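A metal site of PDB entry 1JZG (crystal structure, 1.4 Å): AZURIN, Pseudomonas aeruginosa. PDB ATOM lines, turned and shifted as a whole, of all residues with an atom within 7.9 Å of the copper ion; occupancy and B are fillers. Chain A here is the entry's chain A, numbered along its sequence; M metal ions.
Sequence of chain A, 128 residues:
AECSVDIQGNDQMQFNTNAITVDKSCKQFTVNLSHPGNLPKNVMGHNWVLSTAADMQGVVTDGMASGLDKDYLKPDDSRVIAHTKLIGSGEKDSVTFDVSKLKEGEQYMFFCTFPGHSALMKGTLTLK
Phe 114 touches the copper ion.
Met 121 touches the copper ion (SD to CU, 3.3 Å).
Within 4 Å of the copper ion: Gly 45, His 46, Cys 112, Phe 114, His 117 and Met 121.
The copper ion is bound by ND1 of His 46, ND1 of His 117 and SG of Cys 112.
The copper ion has three donor atoms within binding distance.
Slightly farther from the copper ion lies the backbone carbonyl oxygen (O) of Gly 45 (2.7 Å).
ND1 of His 46 lies close to SD of Met 121.
The backbone carbonyl oxygen (O) of Asn 10 is in hydrogen-bond range of a ring nitrogen (NE2) of His 46.
The backbone carbonyl oxygen (O) of His 46 lies within hydrogen-bond range of the backbone NH (N) of Ile 87, 2.8 Å away.
The backbone carbonyl oxygen of Gly 45 lies close to a ring nitrogen (ND1) of His 117 (3.4 Å).
The backbone carbonyl oxygen (O) of Gly 45 sits close to the side-chain sulfur (SG) of Cys 112 (3.7 Å).
The backbone carbonyl oxygen of Met 121 sits at hydrogen-bond distance from the backbone NH of Cys 112 (3.1 Å).
SG of Cys 112 lies close to N of Phe 114.
OD1 of Asn 47 lies close to SG of Cys 112, 3.5 Å away.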
ATOM      1  N   GLY A   9      32.948 -14.400  -5.831  1.00  0.00           N
ATOM      2  CA  GLY A   9      32.914 -12.956  -5.930  1.00  0.00           C
ATOM      3  C   GLY A   9      33.366 -12.571  -4.533  1.00  0.00           C
ATOM      4  O   GLY A   9      32.795 -13.069  -3.563  1.00  0.00           O
ATOM      5  N   ASN A  10      34.356 -11.704  -4.391  1.00  0.00           N
ATOM      6  CA  ASN A  10      34.861 -11.374  -3.050  1.00  0.00           C
ATOM      7  C   ASN A  10      34.784  -9.893  -2.632  1.00  0.00           C
ATOM      8  O   ASN A  10      34.155  -9.094  -3.319  1.00  0.00           O
ATOM      9  CB  ASN A  10      36.303 -11.889  -2.936  1.00  0.00           C
ATOM     10  CG  ASN A  10      37.250 -11.188  -3.891  1.00  0.00           C
ATOM     11  OD1 ASN A  10      36.951 -10.101  -4.390  1.00  0.00           O
ATOM     12  ND2 ASN A  10      38.402 -11.789  -4.126  1.00  0.00           N
ATOM     13  N   MET A  13      35.950  -6.947  -4.967  1.00  0.00           N
ATOM     14  CA  MET A  13      35.109  -6.686  -6.140  1.00  0.00           C
ATOM     15  C   MET A  13      35.660  -7.371  -7.396  1.00  0.00           C
ATOM     16  O   MET A  13      35.753  -6.761  -8.467  1.00  0.00           O
ATOM     17  CB  MET A  13      34.983  -5.165  -6.351  1.00  0.00           C
ATOM     18  CG  MET A  13      33.781  -4.720  -7.150  1.00  0.00           C
ATOM     19  SD  MET A  13      33.742  -2.928  -7.354  1.00  0.00           S
ATOM     20  CE  MET A  13      35.062  -2.744  -8.545  1.00  0.00           C
ATOM     21  N   GLN A  14      36.008  -8.642  -7.255  1.00  0.00           N
ATOM     22  CA  GLN A  14      36.542  -9.443  -8.335  1.00  0.00           C
ATOM     23  C   GLN A  14      35.946 -10.850  -8.352  1.00  0.00           C
ATOM     24  O   GLN A  14      35.622 -11.399  -7.304  1.00  0.00           O
ATOM     25  CB  GLN A  14      38.079  -9.594  -8.215  1.00  0.00           C
ATOM     26  CG  GLN A  14      38.863  -8.292  -8.368  1.00  0.00           C
ATOM     27  CD  GLN A  14      40.379  -8.473  -8.365  1.00  0.00           C
ATOM     28  OE1 GLN A  14      41.040  -8.261  -9.391  1.00  0.00           O
ATOM     29  NE2 GLN A  14      40.948  -8.808  -7.213  1.00  0.00           N
ATOM     30  N   PHE A  15      35.749 -11.378  -9.556  1.00  0.00           N
ATOM     31  CA  PHE A  15      35.284 -12.747  -9.716  1.00  0.00           C
ATOM     32  C   PHE A  15      36.618 -13.491  -9.844  1.00  0.00           C
ATOM     33  O   PHE A  15      37.652 -12.861 -10.130  1.00  0.00           O
ATOM     34  CB  PHE A  15      34.537 -12.952 -11.053  1.00  0.00           C
ATOM     35  CG  PHE A  15      33.091 -12.559 -11.033  1.00  0.00           C
ATOM     36  CD1 PHE A  15      32.215 -13.050 -10.069  1.00  0.00           C
ATOM     37  CD2 PHE A  15      32.590 -11.762 -12.058  1.00  0.00           C
ATOM     38  CE1 PHE A  15      30.845 -12.758 -10.149  1.00  0.00           C
ATOM     39  CE2 PHE A  15      31.228 -11.471 -12.144  1.00  0.00           C
ATOM     40  CZ  PHE A  15      30.359 -11.973 -11.186  1.00  0.00           C
ATOM     41  N   LEU A  33      27.957 -19.989  -7.784  1.00  0.00           N
ATOM     42  CA  LEU A  33      28.546 -18.763  -7.237  1.00  0.00           C
ATOM     43  C   LEU A  33      28.581 -18.764  -5.713  1.00  0.00           C
ATOM     44  O   LEU A  33      27.631 -19.199  -5.064  1.00  0.00           O
ATOM     45  CB  LEU A  33      27.722 -17.555  -7.687  1.00  0.00           C
ATOM     46  CG  LEU A  33      28.236 -16.193  -7.211  1.00  0.00           C
ATOM     47  CD1 LEU A  33      29.517 -15.847  -7.934  1.00  0.00           C
ATOM     48  CD2 LEU A  33      27.184 -15.122  -7.452  1.00  0.00           C
ATOM     49  N   HIS A  35      30.378 -16.391  -2.119  1.00  0.00           N
ATOM     50  CA  HIS A  35      30.940 -15.114  -1.688  1.00  0.00           C
ATOM     51  C   HIS A  35      31.836 -15.332  -0.464  1.00  0.00           C
ATOM     52  O   HIS A  35      31.349 -15.383   0.664  1.00  0.00           O
ATOM     53  CB  HIS A  35      29.787 -14.170  -1.342  1.00  0.00           C
ATOM     54  CG  HIS A  35      30.184 -12.740  -1.213  1.00  0.00           C
ATOM     55  ND1 HIS A  35      31.308 -12.315  -0.522  1.00  0.00           N
ATOM     56  CD2 HIS A  35      29.578 -11.606  -1.652  1.00  0.00           C
ATOM     57  CE1 HIS A  35      31.363 -11.004  -0.536  1.00  0.00           C
ATOM     58  NE2 HIS A  35      30.326 -10.548  -1.216  1.00  0.00           N
ATOM     59  N   LYS A  41      25.432  -8.168   1.370  1.00  0.00           N
ATOM     60  CA  LYS A  41      25.012  -7.899  -0.008  1.00  0.00           C
ATOM     61  C   LYS A  41      24.586  -6.478  -0.323  1.00  0.00           C
ATOM     62  O   LYS A  41      24.544  -6.086  -1.494  1.00  0.00           O
ATOM     63  CB  LYS A  41      23.947  -8.894  -0.481  1.00  0.00           C
ATOM     64  CG  LYS A  41      22.551  -8.670   0.052  1.00  0.00           C
ATOM     65  CD  LYS A  41      21.549  -9.524  -0.708  1.00  0.00           C
ATOM     66  CE  LYS A  41      20.170  -9.415  -0.079  1.00  0.00           C
ATOM     67  NZ  LYS A  41      19.187 -10.319  -0.717  1.00  0.00           N
ATOM     68  N   VAL A  43      26.286  -3.848   0.496  1.00  0.00           N
ATOM     69  CA  VAL A  43      27.472  -3.041   0.231  1.00  0.00           C
ATOM     70  C   VAL A  43      28.431  -3.713  -0.750  1.00  0.00           C
ATOM     71  O   VAL A  43      29.141  -3.027  -1.501  1.00  0.00           O
ATOM     72  CB  VAL A  43      28.258  -2.698   1.525  1.00  0.00           C
ATOM     73  CG1 VAL A  43      27.356  -2.015   2.547  1.00  0.00           C
ATOM     74  CG2 VAL A  43      28.903  -3.936   2.124  1.00  0.00           C
ATOM     75  N   MET A  44      28.433  -5.046  -0.776  1.00  0.00           N
ATOM     76  CA  MET A  44      29.314  -5.800  -1.658  1.00  0.00           C
ATOM     77  C   MET A  44      28.599  -7.045  -2.201  1.00  0.00           C
ATOM     78  O   MET A  44      29.164  -8.143  -2.282  1.00  0.00           O
ATOM     79  CB  MET A  44      30.596  -6.185  -0.898  1.00  0.00           C
ATOM     80  CG  MET A  44      31.712  -6.829  -1.713  1.00  0.00           C
ATOM     81  SD  MET A  44      32.408  -5.785  -3.014  1.00  0.00           S
ATOM     82  CE  MET A  44      33.111  -4.453  -2.041  1.00  0.00           C
ATOM     83  N   GLY A  45      27.338  -6.864  -2.586  1.00  0.00           N
ATOM     84  CA  GLY A  45      26.555  -7.960  -3.123  1.00  0.00           C
ATOM     85  C   GLY A  45      26.994  -8.312  -4.531  1.00  0.00           C
ATOM     86  O   GLY A  45      27.423  -7.458  -5.306  1.00  0.00           O
ATOM     87  N   HIS A  46      26.924  -9.597  -4.858  1.00  0.00           N
ATOM     88  CA  HIS A  46      27.316 -10.069  -6.175  1.00  0.00           C
ATOM     89  C   HIS A  46      26.326 -11.046  -6.758  1.00  0.00           C
ATOM     90  O   HIS A  46      25.767 -11.890  -6.055  1.00  0.00           O
ATOM     91  CB  HIS A  46      28.653 -10.816  -6.130  1.00  0.00           C
ATOM     92  CG  HIS A  46      29.792 -10.034  -5.567  1.00  0.00           C
ATOM     93  ND1 HIS A  46      30.069  -8.742  -5.938  1.00  0.00           N
ATOM     94  CD2 HIS A  46      30.755 -10.393  -4.687  1.00  0.00           C
ATOM     95  CE1 HIS A  46      31.157  -8.329  -5.309  1.00  0.00           C
ATOM     96  NE2 HIS A  46      31.589  -9.315  -4.548  1.00  0.00           N
ATOM     97  N   ASN A  47      26.101 -10.912  -8.059  1.00  0.00           N
ATOM     98  CA  ASN A  47      25.283 -11.861  -8.798  1.00  0.00           C
ATOM     99  C   ASN A  47      26.088 -12.230 -10.041  1.00  0.00           C
ATOM    100  O   ASN A  47      27.147 -11.644 -10.299  1.00  0.00           O
ATOM    101  CB  ASN A  47      23.864 -11.340  -9.143  1.00  0.00           C
ATOM    102  CG  ASN A  47      23.856 -10.013  -9.868  1.00  0.00           C
ATOM    103  OD1 ASN A  47      24.890  -9.521 -10.325  1.00  0.00           O
ATOM    104  ND2 ASN A  47      22.676  -9.408  -9.984  1.00  0.00           N
ATOM    105  N   TRP A  48      25.662 -13.290 -10.709  1.00  0.00           N
ATOM    106  CA  TRP A  48      26.303 -13.751 -11.936  1.00  0.00           C
ATOM    107  C   TRP A  48      25.179 -13.659 -12.952  1.00  0.00           C
ATOM    108  O   TRP A  48      24.198 -14.401 -12.885  1.00  0.00           O
ATOM    109  CB  TRP A  48      26.805 -15.194 -11.798  1.00  0.00           C
ATOM    110  CG  TRP A  48      27.556 -15.695 -13.012  1.00  0.00           C
ATOM    111  CD1 TRP A  48      28.897 -15.560 -13.236  1.00  0.00           C
ATOM    112  CD2 TRP A  48      27.002 -16.369 -14.133  1.00  0.00           C
ATOM    113  NE1 TRP A  48      29.212 -16.124 -14.452  1.00  0.00           N
ATOM    114  CE2 TRP A  48      28.068 -16.635 -15.030  1.00  0.00           C
ATOM    115  CE3 TRP A  48      25.721 -16.784 -14.488  1.00  0.00           C
ATOM    116  CZ2 TRP A  48      27.887 -17.287 -16.250  1.00  0.00           C
ATOM    117  CZ3 TRP A  48      25.532 -17.435 -15.702  1.00  0.00           C
ATOM    118  CH2 TRP A  48      26.612 -17.685 -16.572  1.00  0.00           C
ATOM    119  N   LEU A  86      21.389 -12.252  -6.104  1.00  0.00           N
ATOM    120  CA  LEU A  86      22.446 -11.416  -5.541  1.00  0.00           C
ATOM    121  C   LEU A  86      22.747 -11.998  -4.156  1.00  0.00           C
ATOM    122  O   LEU A  86      21.834 -12.224  -3.362  1.00  0.00           O
ATOM    123  CB  LEU A  86      21.956  -9.968  -5.401  1.00  0.00           C
ATOM    124  CG  LEU A  86      22.984  -8.886  -5.071  1.00  0.00           C
ATOM    125  CD1 LEU A  86      23.681  -8.447  -6.348  1.00  0.00           C
ATOM    126  CD2 LEU A  86      22.308  -7.689  -4.432  1.00  0.00           C
ATOM    127  N   ILE A  87      24.031 -12.245  -3.882  1.00  0.00           N
ATOM    128  CA  ILE A  87      24.443 -12.815  -2.600  1.00  0.00           C
ATOM    129  C   ILE A  87      25.510 -11.986  -1.900  1.00  0.00           C
ATOM    130  O   ILE A  87      26.245 -11.218  -2.521  1.00  0.00           O
ATOM    131  CB  ILE A  87      24.988 -14.253  -2.770  1.00  0.00           C
ATOM    132  CG1 ILE A  87      26.256 -14.254  -3.631  1.00  0.00           C
ATOM    133  CG2 ILE A  87      23.929 -15.167  -3.370  1.00  0.00           C
ATOM    134  CD1 ILE A  87      26.930 -15.594  -3.753  1.00  0.00           C
ATOM    135  N   PHE A 111      28.553 -10.986 -15.803  1.00  0.00           N
ATOM    136  CA  PHE A 111      28.925  -9.827 -15.001  1.00  0.00           C
ATOM    137  C   PHE A 111      28.016  -9.705 -13.797  1.00  0.00           C
ATOM    138  O   PHE A 111      26.989 -10.386 -13.711  1.00  0.00           O
ATOM    139  CB  PHE A 111      28.769  -8.539 -15.840  1.00  0.00           C
ATOM    140  CG  PHE A 111      27.482  -8.498 -16.647  1.00  0.00           C
ATOM    141  CD1 PHE A 111      27.427  -9.057 -17.918  1.00  0.00           C
ATOM    142  CD2 PHE A 111      26.318  -7.941 -16.111  1.00  0.00           C
ATOM    143  CE1 PHE A 111      26.245  -9.066 -18.646  1.00  0.00           C
ATOM    144  CE2 PHE A 111      25.120  -7.941 -16.840  1.00  0.00           C
ATOM    145  CZ  PHE A 111      25.095  -8.509 -18.110  1.00  0.00           C
ATOM    146  N   CYS A 112      28.412  -8.850 -12.875  1.00  0.00           N
ATOM    147  CA  CYS A 112      27.648  -8.565 -11.669  1.00  0.00           C
ATOM    148  C   CYS A 112      26.981  -7.237 -11.946  1.00  0.00           C
ATOM    149  O   CYS A 112      27.615  -6.322 -12.495  1.00  0.00           O
ATOM    150  CB  CYS A 112      28.567  -8.417 -10.453  1.00  0.00           C
ATOM    151  SG  CYS A 112      27.700  -7.901  -8.961  1.00  0.00           S
ATOM    152  N   THR A 113      25.709  -7.098 -11.565  1.00  0.00           N
ATOM    153  CA  THR A 113      24.985  -5.848 -11.793  1.00  0.00           C
ATOM    154  C   THR A 113      24.872  -4.934 -10.576  1.00  0.00           C
ATOM    155  O   THR A 113      24.161  -3.927 -10.616  1.00  0.00           O
ATOM    156  CB  THR A 113      23.580  -6.087 -12.397  1.00  0.00           C
ATOM    157  OG1 THR A 113      22.811  -6.908 -11.510  1.00  0.00           O
ATOM    158  CG2 THR A 113      23.682  -6.771 -13.757  1.00  0.00           C
ATOM    159  N   PHE A 114      25.540  -5.278  -9.467  1.00  0.00           N
ATOM    160  CA  PHE A 114      25.507  -4.406  -8.295  1.00  0.00           C
ATOM    161  C   PHE A 114      26.150  -3.106  -8.784  1.00  0.00           C
ATOM    162  O   PHE A 114      27.102  -3.137  -9.559  1.00  0.00           O
ATOM    163  CB  PHE A 114      26.342  -4.997  -7.155  1.00  0.00           C
ATOM    164  CG  PHE A 114      26.288  -4.212  -5.882  1.00  0.00           C
ATOM    165  CD1 PHE A 114      27.121  -3.115  -5.689  1.00  0.00           C
ATOM    166  CD2 PHE A 114      25.373  -4.549  -4.885  1.00  0.00           C
ATOM    167  CE1 PHE A 114      27.053  -2.359  -4.527  1.00  0.00           C
ATOM    168  CE2 PHE A 114      25.299  -3.802  -3.714  1.00  0.00           C
ATOM    169  CZ  PHE A 114      26.139  -2.706  -3.528  1.00  0.00           C
ATOM    170  N   PRO A 115      25.650  -1.945  -8.333  1.00  0.00           N
ATOM    171  CA  PRO A 115      26.217  -0.653  -8.771  1.00  0.00           C
ATOM    172  C   PRO A 115      27.745  -0.525  -8.809  1.00  0.00           C
ATOM    173  O   PRO A 115      28.425  -0.650  -7.791  1.00  0.00           O
ATOM    174  CB  PRO A 115      25.597   0.336  -7.806  1.00  0.00           C
ATOM    175  CG  PRO A 115      24.244  -0.229  -7.600  1.00  0.00           C
ATOM    176  CD  PRO A 115      24.530  -1.709  -7.404  1.00  0.00           C
ATOM    177  N   GLY A 116      28.239  -0.295 -10.030  1.00  0.00           N
ATOM    178  CA  GLY A 116      29.660  -0.107 -10.277  1.00  0.00           C
ATOM    179  C   GLY A 116      30.532  -1.333 -10.411  1.00  0.00           C
ATOM    180  O   GLY A 116      31.622  -1.262 -10.989  1.00  0.00           O
ATOM    181  N   HIS A 117      30.047  -2.471  -9.935  1.00  0.00           N
ATOM    182  CA  HIS A 117      30.842  -3.688  -9.977  1.00  0.00           C
ATOM    183  C   HIS A 117      31.280  -4.213 -11.329  1.00  0.00           C
ATOM    184  O   HIS A 117      32.379  -4.738 -11.440  1.00  0.00           O
ATOM    185  CB  HIS A 117      30.162  -4.791  -9.190  1.00  0.00           C
ATOM    186  CG  HIS A 117      30.173  -4.579  -7.720  1.00  0.00           C
ATOM    187  ND1 HIS A 117      29.805  -5.551  -6.819  1.00  0.00           N
ATOM    188  CD2 HIS A 117      30.493  -3.495  -6.977  1.00  0.00           C
ATOM    189  CE1 HIS A 117      29.887  -5.089  -5.597  1.00  0.00           C
ATOM    190  NE2 HIS A 117      30.313  -3.829  -5.663  1.00  0.00           N
ATOM    191  N   SER A 118      30.441  -4.050 -12.351  1.00  0.00           N
ATOM    192  CA  SER A 118      30.795  -4.577 -13.674  1.00  0.00           C
ATOM    193  C   SER A 118      32.062  -4.004 -14.303  1.00  0.00           C
ATOM    194  O   SER A 118      32.573  -4.563 -15.256  1.00  0.00           O
ATOM    195  CB  SER A 118      29.608  -4.482 -14.640  1.00  0.00           C
ATOM    196  OG  SER A 118      29.399  -3.157 -15.084  1.00  0.00           O
ATOM    197  N   MET A 121      34.047  -6.721 -12.442  1.00  0.00           N
ATOM    198  CA  MET A 121      33.351  -7.992 -12.386  1.00  0.00           C
ATOM    199  C   MET A 121      32.594  -8.338 -13.651  1.00  0.00           C
ATOM    200  O   MET A 121      31.372  -8.219 -13.740  1.00  0.00           O
ATOM    201  CB  MET A 121      32.427  -8.041 -11.169  1.00  0.00           C
ATOM    202  CG  MET A 121      33.202  -7.841  -9.875  1.00  0.00           C
ATOM    203  SD  MET A 121      32.254  -8.080  -8.370  1.00  0.00           S
ATOM    204  CE  MET A 121      32.055  -9.876  -8.400  1.00  0.00           C
HETATM  205 CU    CU M   1      29.170  -7.514  -7.321  1.00  0.00          CU
